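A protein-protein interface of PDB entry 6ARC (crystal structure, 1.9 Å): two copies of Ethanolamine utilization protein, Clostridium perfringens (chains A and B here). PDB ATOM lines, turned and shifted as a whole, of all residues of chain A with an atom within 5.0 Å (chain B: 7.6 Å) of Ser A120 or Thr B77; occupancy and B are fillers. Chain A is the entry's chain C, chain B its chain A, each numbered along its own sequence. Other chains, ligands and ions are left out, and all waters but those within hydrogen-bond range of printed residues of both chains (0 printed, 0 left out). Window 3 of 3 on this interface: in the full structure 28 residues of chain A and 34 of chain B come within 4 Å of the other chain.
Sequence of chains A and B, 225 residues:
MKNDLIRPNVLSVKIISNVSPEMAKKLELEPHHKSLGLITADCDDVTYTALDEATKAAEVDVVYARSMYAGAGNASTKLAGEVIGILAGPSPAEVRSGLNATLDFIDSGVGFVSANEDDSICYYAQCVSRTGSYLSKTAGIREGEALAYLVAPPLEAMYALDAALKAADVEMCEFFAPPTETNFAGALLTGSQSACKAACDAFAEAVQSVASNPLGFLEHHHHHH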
ATOM      1  N   ASN A 116     -10.805   2.614  16.695  1.00  0.00           N
ATOM      2  CA  ASN A 116     -12.005   1.988  16.158  1.00  0.00           C
ATOM      3  C   ASN A 116     -11.817   0.480  16.044  1.00  0.00           C
ATOM      4  O   ASN A 116     -10.776  -0.083  16.401  1.00  0.00           O
ATOM      5  CB  ASN A 116     -12.406   2.616  14.823  1.00  0.00           C
ATOM      6  CG  ASN A 116     -11.383   2.421  13.729  1.00  0.00           C
ATOM      7  OD1 ASN A 116     -10.408   1.690  13.875  1.00  0.00           O
ATOM      8  ND2 ASN A 116     -11.632   3.064  12.597  1.00  0.00           N
ATOM      9  N   ASP A 118     -11.638  -1.827  13.624  1.00  0.00           N
ATOM     10  CA  ASP A 118     -10.686  -2.486  12.741  1.00  0.00           C
ATOM     11  C   ASP A 118      -9.320  -1.819  12.759  1.00  0.00           C
ATOM     12  O   ASP A 118      -8.490  -2.106  11.907  1.00  0.00           O
ATOM     13  CB  ASP A 118     -11.239  -2.564  11.314  1.00  0.00           C
ATOM     14  CG  ASP A 118     -11.347  -1.218  10.647  1.00  0.00           C
ATOM     15  OD1 ASP A 118     -11.117  -0.200  11.331  1.00  0.00           O
ATOM     16  OD2 ASP A 118     -11.713  -1.172   9.445  1.00  0.00           O
ATOM     17  N   ASP A 119      -9.071  -0.945  13.717  1.00  0.00           N
ATOM     18  CA  ASP A 119      -7.757  -0.334  13.900  1.00  0.00           C
ATOM     19  C   ASP A 119      -7.315   0.452  12.673  1.00  0.00           C
ATOM     20  O   ASP A 119      -6.119   0.611  12.417  1.00  0.00           O
ATOM     21  CB  ASP A 119      -6.720  -1.398  14.270  1.00  0.00           C
ATOM     22  CG  ASP A 119      -7.156  -2.259  15.483  1.00  0.00           C
ATOM     23  OD1 ASP A 119      -7.919  -1.764  16.354  1.00  0.00           O
ATOM     24  OD2 ASP A 119      -6.744  -3.443  15.548  1.00  0.00           O
ATOM     25  N   SER A 120      -8.277   1.010  11.946  1.00  0.00           N
ATOM     26  CA  SER A 120      -7.995   1.822  10.770  1.00  0.00           C
ATOM     27  C   SER A 120      -7.920   3.311  11.086  1.00  0.00           C
ATOM     28  O   SER A 120      -7.683   4.107  10.187  1.00  0.00           O
ATOM     29  CB  SER A 120      -9.049   1.574   9.691  1.00  0.00           C
ATOM     30  OG  SER A 120     -10.329   1.903  10.172  1.00  0.00           O
ATOM     31  N   ILE A 121      -8.143   3.707  12.329  1.00  0.00           N
ATOM     32  CA  ILE A 121      -7.779   5.026  12.826  1.00  0.00           C
ATOM     33  C   ILE A 121      -6.948   4.767  14.077  1.00  0.00           C
ATOM     34  O   ILE A 121      -7.335   3.950  14.924  1.00  0.00           O
ATOM     35  CB  ILE A 121      -8.995   5.923  13.152  1.00  0.00           C
ATOM     36  CG1 ILE A 121      -9.854   6.149  11.919  1.00  0.00           C
ATOM     37  CG2 ILE A 121      -8.536   7.291  13.704  1.00  0.00           C
ATOM     38  CD1 ILE A 121     -11.165   6.811  12.196  1.00  0.00           C
ATOM     39  N   CYS A 122      -5.793   5.421  14.170  1.00  0.00           N
ATOM     40  CA  CYS A 122      -4.925   5.250  15.323  1.00  0.00           C
ATOM     41  C   CYS A 122      -4.184   6.550  15.589  1.00  0.00           C
ATOM     42  O   CYS A 122      -4.087   7.431  14.725  1.00  0.00           O
ATOM     43  CB  CYS A 122      -3.938   4.115  15.108  1.00  0.00           C
ATOM     44  SG  CYS A 122      -2.942   4.439  13.660  1.00  0.00           S
ATOM     45  N   PRO A 153      -3.873  11.104  12.280  1.00  0.00           N
ATOM     46  CA  PRO A 153      -4.041  11.420  10.869  1.00  0.00           C
ATOM     47  C   PRO A 153      -4.448  12.870  10.707  1.00  0.00           C
ATOM     48  O   PRO A 153      -4.839  13.522  11.684  1.00  0.00           O
ATOM     49  CB  PRO A 153      -5.141  10.455  10.400  1.00  0.00           C
ATOM     50  CG  PRO A 153      -5.078   9.316  11.374  1.00  0.00           C
ATOM     51  CD  PRO A 153      -4.705   9.958  12.697  1.00  0.00           C
ATOM     52  N   PHE A 184       0.667  11.361   8.378  1.00  0.00           N
ATOM     53  CA  PHE A 184       0.172  11.753   9.684  1.00  0.00           C
ATOM     54  C   PHE A 184       0.508  13.224   9.907  1.00  0.00           C
ATOM     55  O   PHE A 184       1.004  13.928   9.000  1.00  0.00           O
ATOM     56  CB  PHE A 184       0.766  10.843  10.759  1.00  0.00           C
ATOM     57  CG  PHE A 184       0.081   9.504  10.873  1.00  0.00           C
ATOM     58  CD1 PHE A 184       0.310   8.507   9.945  1.00  0.00           C
ATOM     59  CD2 PHE A 184      -0.796   9.259  11.912  1.00  0.00           C
ATOM     60  CE1 PHE A 184      -0.328   7.267  10.051  1.00  0.00           C
ATOM     61  CE2 PHE A 184      -1.444   8.045  12.031  1.00  0.00           C
ATOM     62  CZ  PHE A 184      -1.204   7.025  11.091  1.00  0.00           C
ATOM     63  N   LEU B  11     -14.726  12.345   3.575  1.00  0.00           N
ATOM     64  CA  LEU B  11     -14.467  11.399   4.653  1.00  0.00           C
ATOM     65  C   LEU B  11     -14.632  12.004   6.034  1.00  0.00           C
ATOM     66  O   LEU B  11     -15.126  11.323   6.940  1.00  0.00           O
ATOM     67  CB  LEU B  11     -13.050  10.824   4.527  1.00  0.00           C
ATOM     68  CG  LEU B  11     -12.765  10.147   3.186  1.00  0.00           C
ATOM     69  CD1 LEU B  11     -11.282   9.769   3.084  1.00  0.00           C
ATOM     70  CD2 LEU B  11     -13.644   8.938   3.000  1.00  0.00           C
ATOM     71  N   ALA B  72      -5.224   8.235  -2.387  1.00  0.00           N
ATOM     72  CA  ALA B  72      -6.219   7.705  -1.459  1.00  0.00           C
ATOM     73  C   ALA B  72      -6.200   6.181  -1.413  1.00  0.00           C
ATOM     74  O   ALA B  72      -6.486   5.587  -0.365  1.00  0.00           O
ATOM     75  CB  ALA B  72      -7.617   8.186  -1.867  1.00  0.00           C
ATOM     76  N   ASN B  74      -3.737   4.316  -1.332  1.00  0.00           N
ATOM     77  CA  ASN B  74      -2.662   3.883  -0.457  1.00  0.00           C
ATOM     78  C   ASN B  74      -2.762   4.476   0.940  1.00  0.00           C
ATOM     79  O   ASN B  74      -1.791   4.395   1.693  1.00  0.00           O
ATOM     80  CB  ASN B  74      -1.317   4.253  -1.078  1.00  0.00           C
ATOM     81  CG  ASN B  74      -1.032   3.432  -2.344  1.00  0.00           C
ATOM     82  OD1 ASN B  74      -1.147   2.219  -2.331  1.00  0.00           O
ATOM     83  ND2 ASN B  74      -0.699   4.099  -3.432  1.00  0.00           N
ATOM     84  N   ALA B  75      -3.896   5.098   1.284  1.00  0.00           N
ATOM     85  CA  ALA B  75      -4.098   5.628   2.630  1.00  0.00           C
ATOM     86  C   ALA B  75      -4.003   4.529   3.681  1.00  0.00           C
ATOM     87  O   ALA B  75      -4.546   3.433   3.522  1.00  0.00           O
ATOM     88  CB  ALA B  75      -5.463   6.314   2.728  1.00  0.00           C
ATOM     89  N   SER B  76      -3.302   4.825   4.767  1.00  0.00           N
ATOM     90  CA  SER B  76      -3.165   3.846   5.834  1.00  0.00           C
ATOM     91  C   SER B  76      -4.237   3.993   6.907  1.00  0.00           C
ATOM     92  O   SER B  76      -4.431   3.068   7.697  1.00  0.00           O
ATOM     93  CB  SER B  76      -1.791   3.956   6.486  1.00  0.00           C
ATOM     94  OG  SER B  76      -1.657   5.142   7.231  1.00  0.00           O
ATOM     95  N   THR B  77      -4.943   5.113   6.952  1.00  0.00           N
ATOM     96  CA  THR B  77      -6.006   5.281   7.922  1.00  0.00           C
ATOM     97  C   THR B  77      -7.275   5.687   7.184  1.00  0.00           C
ATOM     98  O   THR B  77      -7.236   6.135   6.034  1.00  0.00           O
ATOM     99  CB  THR B  77      -5.629   6.316   8.996  1.00  0.00           C
ATOM    100  OG1 THR B  77      -5.453   7.609   8.391  1.00  0.00           O
ATOM    101  CG2 THR B  77      -4.320   5.876   9.752  1.00  0.00           C
ATOM    102  N   LYS B  78      -8.399   5.549   7.883  1.00  0.00           N
ATOM    103  CA  LYS B  78      -9.726   5.625   7.268  1.00  0.00           C
ATOM    104  C   LYS B  78     -10.110   7.034   6.807  1.00  0.00           C
ATOM    105  O   LYS B  78     -10.848   7.180   5.821  1.00  0.00           O
ATOM    106  CB  LYS B  78     -10.755   5.087   8.273  1.00  0.00           C
ATOM    107  CG  LYS B  78     -12.214   5.142   7.845  1.00  0.00           C
ATOM    108  CD  LYS B  78     -13.134   4.630   8.977  1.00  0.00           C
ATOM    109  CE  LYS B  78     -14.595   4.825   8.679  1.00  0.00           C
ATOM    110  NZ  LYS B  78     -15.035   4.112   7.444  1.00  0.00           N
ATOM    111  N   LEU B  79      -9.672   8.073   7.515  1.00  0.00           N
ATOM    112  CA  LEU B  79     -10.120   9.437   7.265  1.00  0.00           C
ATOM    113  C   LEU B  79      -9.060  10.293   6.579  1.00  0.00           C
ATOM    114  O   LEU B  79      -9.309  11.473   6.325  1.00  0.00           O
ATOM    115  CB  LEU B  79     -10.552  10.092   8.589  1.00  0.00           C
ATOM    116  CG  LEU B  79     -11.562   9.327   9.450  1.00  0.00           C
ATOM    117  CD1 LEU B  79     -11.894  10.111  10.725  1.00  0.00           C
ATOM    118  CD2 LEU B  79     -12.858   9.056   8.731  1.00  0.00           C
ATOM    119  N   ALA B  80      -7.883   9.740   6.270  1.00  0.00           N
ATOM    120  CA  ALA B  80      -6.836  10.551   5.656  1.00  0.00           C
ATOM    121  C   ALA B  80      -7.140  10.819   4.183  1.00  0.00           C
ATOM    122  O   ALA B  80      -6.884  11.920   3.677  1.00  0.00           O
ATOM    123  CB  ALA B  80      -5.480   9.858   5.820  1.00  0.00           C
ATOM    124  N   GLY B  81      -7.719   9.843   3.497  1.00  0.00           N
ATOM    125  CA  GLY B  81      -8.010  10.018   2.084  1.00  0.00           C
ATOM    126  C   GLY B  81      -6.769  10.456   1.343  1.00  0.00           C
ATOM    127  O   GLY B  81      -5.698   9.873   1.513  1.00  0.00           O
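N of Lys B78 sits at hydrogen-bond distance from O of Ser A120.
N of Ser A120 is in hydrogen-bond range of OD1 of Asn A116, at 3.0 Å. OD1 of Asn A116 is in hydrogen-bond range of N of Ile A121. OD1 of Asp A118 is in hydrogen-bond range of OG of Ser A120, at 2.5 Å.
Among the printed residues, merely in contact across the chains: Ser A120 with Thr B77 (3.1 Å), Pro A153 with Thr B77 (3.5 Å), Phe A184 with Thr B77 (3.6 Å), Ile A121 with Leu B79 (3.7 Å), Phe A184 with Ser B76 (3.8 Å) and Ile A121 with Lys B78 (3.9 Å).
Ser A120 touches just these residues of chain B: Thr B77 and Lys B78. Of the printed residues of chain B, Ile A121 touches Lys B78 and Leu B79. Cys A122 touches none of the printed residues of chain B. Of the printed residues of chain B, Pro A153 touches Thr B77 (3.5 Å). Asn B74 touches none of the printed residues of chain A. Printed residues of chain A within 4 Å of Ser B76: Phe A184 (3.8 Å). Of chain A, only Ser A120, Pro A153 and Phe A184 come within 4 Å of Thr B77. Of the printed residues of chain A, Lys B78 touches Ser A120 and Ile A121. Printed residues of chain A within 4 Å of Leu B79: Ile A121 (3.7 Å). The nearest printed residue of chain B that does not touch Ser A120 is Ser B76 (4.2 Å). The nearest printed residue of chain A that does not touch Thr B77 is Cys A122 (4.4 Å).
Printed residues of chain A that touch a printed residue of chain B: Ser A120, Ile A121, Pro A153 and Phe A184. Hydrophobic or aromatic side chains of chain A within 4 Å of the printed part of chain B: Ile A121, Pro A153 and Phe A184. Hydrophobic or aromatic side chains of chain B within 4 Å of the printed part of chain A: Leu B79. Among the printed residues, 7 pairs touch across the chains.
No position is printed for both chains. Of the 7 pairs that touch across the chains among the printed residues, none has its exchanged pair printed and touching as well.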
